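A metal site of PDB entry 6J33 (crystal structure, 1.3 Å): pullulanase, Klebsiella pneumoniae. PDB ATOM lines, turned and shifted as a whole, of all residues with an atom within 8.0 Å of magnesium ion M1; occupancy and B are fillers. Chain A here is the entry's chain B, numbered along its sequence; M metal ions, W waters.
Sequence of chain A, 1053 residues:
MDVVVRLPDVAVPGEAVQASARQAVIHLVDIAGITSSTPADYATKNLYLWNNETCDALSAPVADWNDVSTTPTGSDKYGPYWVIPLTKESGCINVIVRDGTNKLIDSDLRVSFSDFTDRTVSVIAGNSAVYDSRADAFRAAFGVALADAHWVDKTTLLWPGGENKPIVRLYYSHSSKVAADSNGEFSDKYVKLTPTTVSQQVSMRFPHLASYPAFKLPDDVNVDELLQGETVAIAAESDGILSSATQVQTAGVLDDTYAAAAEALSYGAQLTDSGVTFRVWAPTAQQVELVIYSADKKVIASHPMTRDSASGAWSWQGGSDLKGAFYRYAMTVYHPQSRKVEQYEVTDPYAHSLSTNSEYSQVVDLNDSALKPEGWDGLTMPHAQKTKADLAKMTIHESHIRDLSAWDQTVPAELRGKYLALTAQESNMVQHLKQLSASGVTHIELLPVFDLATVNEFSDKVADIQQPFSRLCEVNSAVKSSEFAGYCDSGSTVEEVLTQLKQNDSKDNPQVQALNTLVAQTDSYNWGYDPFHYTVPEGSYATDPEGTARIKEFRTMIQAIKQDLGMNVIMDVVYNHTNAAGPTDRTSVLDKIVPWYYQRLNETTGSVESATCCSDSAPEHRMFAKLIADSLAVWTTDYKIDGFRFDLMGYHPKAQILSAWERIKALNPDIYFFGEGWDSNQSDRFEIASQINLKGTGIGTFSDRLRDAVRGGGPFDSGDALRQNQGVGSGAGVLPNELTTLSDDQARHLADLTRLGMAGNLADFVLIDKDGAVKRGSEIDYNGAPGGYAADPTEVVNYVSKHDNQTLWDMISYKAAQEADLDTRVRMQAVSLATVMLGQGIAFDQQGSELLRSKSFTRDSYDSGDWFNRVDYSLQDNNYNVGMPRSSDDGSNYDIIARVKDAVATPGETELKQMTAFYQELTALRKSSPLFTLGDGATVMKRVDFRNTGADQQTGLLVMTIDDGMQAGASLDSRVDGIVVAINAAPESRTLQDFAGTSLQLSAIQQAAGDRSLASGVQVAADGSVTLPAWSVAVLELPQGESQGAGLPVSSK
The backbone NH of Gln 1040 lies within hydrogen-bond range of the backbone carbonyl oxygen of Arg 975. The side-chain carboxylate of Asp 973 is in salt-bridge range of the guanidinium group of Arg 975 (3.4 Å). The side-chain carboxylate of Asp 973 is in hydrogen-bond range of the side-chain hydroxyl of Ser 929, 2.6 Å away. The backbone NH of Asp 964 sits at hydrogen-bond distance from the backbone carbonyl oxygen of Asp 977, 2.9 Å away. OD1 of Asp 964 lies within hydrogen-bond range of N of Leu 972. The backbone carbonyl oxygen (O) of Asp 964 lies within hydrogen-bond range of the side-chain amide nitrogen (NE2) of Gln 1044 (2.9 Å). NH1 of Arg 943 is in salt-bridge range of OD1 of Asp 964 (2.8 Å). N of Ser 971 lies close to NE2 of Gln 1044.
Five residues have an atom within 4 Å of magnesium ion M1: Asp 964, Ser 971, Asp 973, Val 976 and Gln 1040. The nearest printed residue that does not touch magnesium ion M1 is Asp 977 (4.03 Å).
Magnesium ion M1 is bound by the side-chain amide oxygen (OE1) of Gln 1040 (2.0 Å). Magnesium ion M1 is bound by the backbone carbonyl oxygen (O) of Asp 973 (2.0 Å). Water W1 is bound to magnesium ion M1 (2.0 Å). OD2 of Asp 964 binds magnesium ion M1 (2.1 Å). The backbone carbonyl oxygen (O) of Val 976 binds magnesium ion M1 (2.1 Å). Magnesium ion M1 is bound by OG of Ser 971, 2.2 Å away.
Water W1 bridges the side-chain carboxylate (OD1) of Asp 977 (2.7 Å) and the backbone carbonyl oxygen (O) of Asp 964 (2.7 Å).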
ATOM      1  N   SER A 929      14.161 -36.248  26.731  1.00  0.00           N
ATOM      2  CA  SER A 929      13.293 -35.485  25.850  1.00  0.00           C
ATOM      3  C   SER A 929      12.162 -36.386  25.365  1.00  0.00           C
ATOM      4  O   SER A 929      12.413 -37.562  25.087  1.00  0.00           O
ATOM      5  CB  SER A 929      14.048 -34.931  24.635  1.00  0.00           C
ATOM      6  OG  SER A 929      13.155 -34.322  23.718  1.00  0.00           O
ATOM      7  N   LEU A 931      11.180 -36.392  22.538  1.00  0.00           N
ATOM      8  CA  LEU A 931      11.473 -36.650  21.129  1.00  0.00           C
ATOM      9  C   LEU A 931      12.057 -38.037  20.883  1.00  0.00           C
ATOM     10  O   LEU A 931      11.913 -38.563  19.785  1.00  0.00           O
ATOM     11  CB  LEU A 931      12.391 -35.570  20.566  1.00  0.00           C
ATOM     12  CG  LEU A 931      11.798 -34.162  20.549  1.00  0.00           C
ATOM     13  CD1 LEU A 931      12.885 -33.159  20.241  1.00  0.00           C
ATOM     14  CD2 LEU A 931      10.711 -34.074  19.504  1.00  0.00           C
ATOM     15  N   ARG A 943       8.923 -36.764  11.817  1.00  0.00           N
ATOM     16  CA  ARG A 943       9.975 -36.104  12.576  1.00  0.00           C
ATOM     17  C   ARG A 943      11.364 -36.724  12.448  1.00  0.00           C
ATOM     18  O   ARG A 943      12.353 -35.990  12.615  1.00  0.00           O
ATOM     19  CB  ARG A 943       9.600 -36.028  14.058  1.00  0.00           C
ATOM     20  CG  ARG A 943       8.388 -35.145  14.335  1.00  0.00           C
ATOM     21  CD  ARG A 943       7.993 -35.172  15.790  1.00  0.00           C
ATOM     22  NE  ARG A 943       6.778 -34.380  16.001  1.00  0.00           N
ATOM     23  CZ  ARG A 943       6.739 -33.188  16.582  1.00  0.00           C
ATOM     24  NH1 ARG A 943       7.855 -32.618  17.029  1.00  0.00           N
ATOM     25  NH2 ARG A 943       5.578 -32.567  16.730  1.00  0.00           N
ATOM     26  N   ASP A 963      12.993 -33.996  14.527  1.00  0.00           N
ATOM     27  CA  ASP A 963      12.530 -32.630  14.329  1.00  0.00           C
ATOM     28  C   ASP A 963      11.549 -32.225  15.410  1.00  0.00           C
ATOM     29  O   ASP A 963      10.627 -32.980  15.745  1.00  0.00           O
ATOM     30  CB  ASP A 963      11.823 -32.533  12.980  1.00  0.00           C
ATOM     31  CG  ASP A 963      11.563 -31.096  12.548  1.00  0.00           C
ATOM     32  OD1 ASP A 963      12.190 -30.174  13.097  1.00  0.00           O
ATOM     33  OD2 ASP A 963      10.712 -30.924  11.635  1.00  0.00           O
ATOM     34  N   ASP A 964      11.742 -31.014  15.953  1.00  0.00           N
ATOM     35  CA  ASP A 964      10.728 -30.353  16.776  1.00  0.00           C
ATOM     36  C   ASP A 964      10.349 -28.989  16.211  1.00  0.00           C
ATOM     37  O   ASP A 964       9.720 -28.181  16.917  1.00  0.00           O
ATOM     38  CB  ASP A 964      11.177 -30.226  18.227  1.00  0.00           C
ATOM     39  CG  ASP A 964      10.000 -30.216  19.199  1.00  0.00           C
ATOM     40  OD1 ASP A 964       9.002 -30.923  18.954  1.00  0.00           O
ATOM     41  OD2 ASP A 964      10.079 -29.469  20.208  1.00  0.00           O
ATOM     42  N   GLY A 965      10.710 -28.706  14.958  1.00  0.00           N
ATOM     43  CA  GLY A 965      10.459 -27.413  14.360  1.00  0.00           C
ATOM     44  C   GLY A 965       9.080 -27.311  13.757  1.00  0.00           C
ATOM     45  O   GLY A 965       8.271 -28.243  13.803  1.00  0.00           O
ATOM     46  N   ALA A 970       3.452 -29.353  16.338  1.00  0.00           N
ATOM     47  CA  ALA A 970       3.673 -28.667  17.600  1.00  0.00           C
ATOM     48  C   ALA A 970       5.065 -28.986  18.143  1.00  0.00           C
ATOM     49  O   ALA A 970       5.666 -30.027  17.840  1.00  0.00           O
ATOM     50  CB  ALA A 970       2.625 -29.091  18.625  1.00  0.00           C
ATOM     51  N   SER A 971       5.589 -28.061  18.949  1.00  0.00           N
ATOM     52  CA  SER A 971       6.807 -28.310  19.703  1.00  0.00           C
ATOM     53  C   SER A 971       6.483 -29.250  20.851  1.00  0.00           C
ATOM     54  O   SER A 971       5.745 -28.893  21.778  1.00  0.00           O
ATOM     55  CB  SER A 971       7.373 -26.997  20.251  1.00  0.00           C
ATOM     56  OG  SER A 971       8.419 -27.232  21.174  1.00  0.00           O
ATOM     57  N   LEU A 972       7.015 -30.478  20.787  1.00  0.00           N
ATOM     58  CA  LEU A 972       6.819 -31.435  21.863  1.00  0.00           C
ATOM     59  C   LEU A 972       7.813 -31.250  23.002  1.00  0.00           C
ATOM     60  O   LEU A 972       7.580 -31.766  24.098  1.00  0.00           O
ATOM     61  CB  LEU A 972       6.892 -32.866  21.310  1.00  0.00           C
ATOM     62  CG  LEU A 972       5.931 -33.221  20.176  1.00  0.00           C
ATOM     63  CD1 LEU A 972       6.224 -34.622  19.669  1.00  0.00           C
ATOM     64  CD2 LEU A 972       4.492 -33.107  20.657  1.00  0.00           C
ATOM     65  N   ASP A 973       8.911 -30.531  22.774  1.00  0.00           N
ATOM     66  CA  ASP A 973       9.939 -30.278  23.783  1.00  0.00           C
ATOM     67  C   ASP A 973      10.193 -28.778  23.778  1.00  0.00           C
ATOM     68  O   ASP A 973      10.711 -28.239  22.800  1.00  0.00           O
ATOM     69  CB  ASP A 973      11.216 -31.045  23.480  1.00  0.00           C
ATOM     70  CG  ASP A 973      12.261 -30.952  24.592  1.00  0.00           C
ATOM     71  OD1 ASP A 973      12.281 -29.940  25.335  1.00  0.00           O
ATOM     72  OD2 ASP A 973      13.074 -31.893  24.731  1.00  0.00           O
ATOM     73  N   SER A 974       9.847 -28.102  24.877  1.00  0.00           N
ATOM     74  CA  SER A 974       9.999 -26.657  24.952  1.00  0.00           C
ATOM     75  C   SER A 974      11.452 -26.214  25.032  1.00  0.00           C
ATOM     76  O   SER A 974      11.725 -25.012  24.851  1.00  0.00           O
ATOM     77  CB  SER A 974       9.219 -26.100  26.146  1.00  0.00           C
ATOM     78  OG  SER A 974       9.494 -26.826  27.323  1.00  0.00           O
ATOM     79  N   ARG A 975      12.396 -27.122  25.286  1.00  0.00           N
ATOM     80  CA  ARG A 975      13.790 -26.734  25.377  1.00  0.00           C
ATOM     81  C   ARG A 975      14.517 -26.761  24.042  1.00  0.00           C
ATOM     82  O   ARG A 975      15.544 -26.093  23.904  1.00  0.00           O
ATOM     83  CB  ARG A 975      14.537 -27.665  26.333  1.00  0.00           C
ATOM     84  CG  ARG A 975      14.240 -27.457  27.802  1.00  0.00           C
ATOM     85  CD  ARG A 975      14.859 -28.597  28.587  1.00  0.00           C
ATOM     86  NE  ARG A 975      14.516 -29.867  27.953  1.00  0.00           N
ATOM     87  CZ  ARG A 975      14.759 -31.066  28.481  1.00  0.00           C
ATOM     88  NH1 ARG A 975      14.396 -32.153  27.816  1.00  0.00           N
ATOM     89  NH2 ARG A 975      15.352 -31.173  29.653  1.00  0.00           N
ATOM     90  N   VAL A 976      14.037 -27.535  23.070  1.00  0.00           N
ATOM     91  CA  VAL A 976      14.771 -27.777  21.836  1.00  0.00           C
ATOM     92  C   VAL A 976      13.852 -27.680  20.628  1.00  0.00           C
ATOM     93  O   VAL A 976      12.659 -27.966  20.695  1.00  0.00           O
ATOM     94  CB  VAL A 976      15.490 -29.154  21.847  1.00  0.00           C
ATOM     95  CG1 VAL A 976      16.356 -29.304  23.091  1.00  0.00           C
ATOM     96  CG2 VAL A 976      14.483 -30.301  21.731  1.00  0.00           C
ATOM     97  N   ASP A 977      14.441 -27.273  19.511  1.00  0.00           N
ATOM     98  CA  ASP A 977      13.795 -27.353  18.213  1.00  0.00           C
ATOM     99  C   ASP A 977      14.165 -28.614  17.454  1.00  0.00           C
ATOM    100  O   ASP A 977      13.624 -28.851  16.376  1.00  0.00           O
ATOM    101  CB  ASP A 977      14.146 -26.120  17.367  1.00  0.00           C
ATOM    102  CG  ASP A 977      13.421 -24.863  17.830  1.00  0.00           C
ATOM    103  OD1 ASP A 977      12.265 -24.954  18.299  1.00  0.00           O
ATOM    104  OD2 ASP A 977      14.007 -23.762  17.704  1.00  0.00           O
ATOM    105  N   GLY A 978      15.067 -29.430  17.991  1.00  0.00           N
ATOM    106  CA  GLY A 978      15.471 -30.650  17.317  1.00  0.00           C
ATOM    107  C   GLY A 978      16.616 -31.308  18.053  1.00  0.00           C
ATOM    108  O   GLY A 978      17.293 -30.655  18.858  1.00  0.00           O
ATOM    109  N   LEU A1038      19.261 -28.483  19.338  1.00  0.00           N
ATOM    110  CA  LEU A1038      19.039 -27.129  18.860  1.00  0.00           C
ATOM    111  C   LEU A1038      18.255 -26.401  19.925  1.00  0.00           C
ATOM    112  O   LEU A1038      17.059 -26.672  20.087  1.00  0.00           O
ATOM    113  CB  LEU A1038      18.228 -27.167  17.569  1.00  0.00           C
ATOM    114  CG  LEU A1038      18.882 -27.593  16.260  1.00  0.00           C
ATOM    115  CD1 LEU A1038      17.848 -27.509  15.149  1.00  0.00           C
ATOM    116  CD2 LEU A1038      20.066 -26.698  15.938  1.00  0.00           C
ATOM    117  N   PRO A1039      18.858 -25.484  20.681  1.00  0.00           N
ATOM    118  CA  PRO A1039      18.114 -24.815  21.759  1.00  0.00           C
ATOM    119  C   PRO A1039      16.952 -24.003  21.193  1.00  0.00           C
ATOM    120  O   PRO A1039      17.086 -23.332  20.175  1.00  0.00           O
ATOM    121  CB  PRO A1039      19.167 -23.919  22.412  1.00  0.00           C
ATOM    122  CG  PRO A1039      20.485 -24.477  21.986  1.00  0.00           C
ATOM    123  CD  PRO A1039      20.255 -25.021  20.609  1.00  0.00           C
ATOM    124  N   GLN A1040      15.809 -24.095  21.866  1.00  0.00           N
ATOM    125  CA  GLN A1040      14.621 -23.391  21.427  1.00  0.00           C
ATOM    126  C   GLN A1040      14.656 -21.964  21.954  1.00  0.00           C
ATOM    127  O   GLN A1040      14.926 -21.739  23.133  1.00  0.00           O
ATOM    128  CB  GLN A1040      13.363 -24.110  21.915  1.00  0.00           C
ATOM    129  CG  GLN A1040      12.058 -23.575  21.322  1.00  0.00           C
ATOM    130  CD  GLN A1040      10.889 -24.531  21.523  1.00  0.00           C
ATOM    131  OE1 GLN A1040      11.064 -25.750  21.503  1.00  0.00           O
ATOM    132  NE2 GLN A1040       9.692 -23.982  21.698  1.00  0.00           N
ATOM    133  N   GLY A1041      14.385 -21.006  21.080  1.00  0.00           N
ATOM    134  CA  GLY A1041      14.376 -19.590  21.417  1.00  0.00           C
ATOM    135  C   GLY A1041      13.046 -19.137  21.965  1.00  0.00           C
ATOM    136  O   GLY A1041      12.308 -19.889  22.603  1.00  0.00           O
ATOM    137  N   SER A1043      10.369 -18.464  20.371  1.00  0.00           N
ATOM    138  CA  SER A1043       9.295 -19.194  19.702  1.00  0.00           C
ATOM    139  C   SER A1043       9.874 -20.440  19.046  1.00  0.00           C
ATOM    140  O   SER A1043      11.095 -20.569  18.881  1.00  0.00           O
ATOM    141  CB  SER A1043       8.587 -18.328  18.655  1.00  0.00           C
ATOM    142  OG  SER A1043       7.970 -17.198  19.256  1.00  0.00           O
ATOM    143  N   GLN A1044       8.986 -21.354  18.660  1.00  0.00           N
ATOM    144  CA  GLN A1044       9.390 -22.565  17.963  1.00  0.00           C
ATOM    145  C   GLN A1044      10.155 -22.205  16.694  1.00  0.00           C
ATOM    146  O   GLN A1044       9.720 -21.334  15.918  1.00  0.00           O
ATOM    147  CB  GLN A1044       8.151 -23.380  17.607  1.00  0.00           C
ATOM    148  CG  GLN A1044       8.441 -24.699  16.890  1.00  0.00           C
ATOM    149  CD  GLN A1044       7.183 -25.405  16.408  1.00  0.00           C
ATOM    150  OE1 GLN A1044       6.150 -24.792  16.181  1.00  0.00           O
ATOM    151  NE2 GLN A1044       7.273 -26.731  16.244  1.00  0.00           N
ATOM    152  N   GLY A1045      11.296 -22.866  16.489  1.00  0.00           N
ATOM    153  CA  GLY A1045      12.189 -22.546  15.401  1.00  0.00           C
ATOM    154  C   GLY A1045      12.024 -23.469  14.204  1.00  0.00           C
ATOM    155  O   GLY A1045      11.067 -24.243  14.099  1.00  0.00           O
HETATM  156 MG    MG M   1      10.606 -27.555  20.899  1.00  0.00          MG
HETATM  157 MG    MG M   2       8.423 -28.406  28.466  1.00  0.00          MG
HETATM  158  O   HOH W   1      10.410 -26.715  19.050  1.00  0.00           O
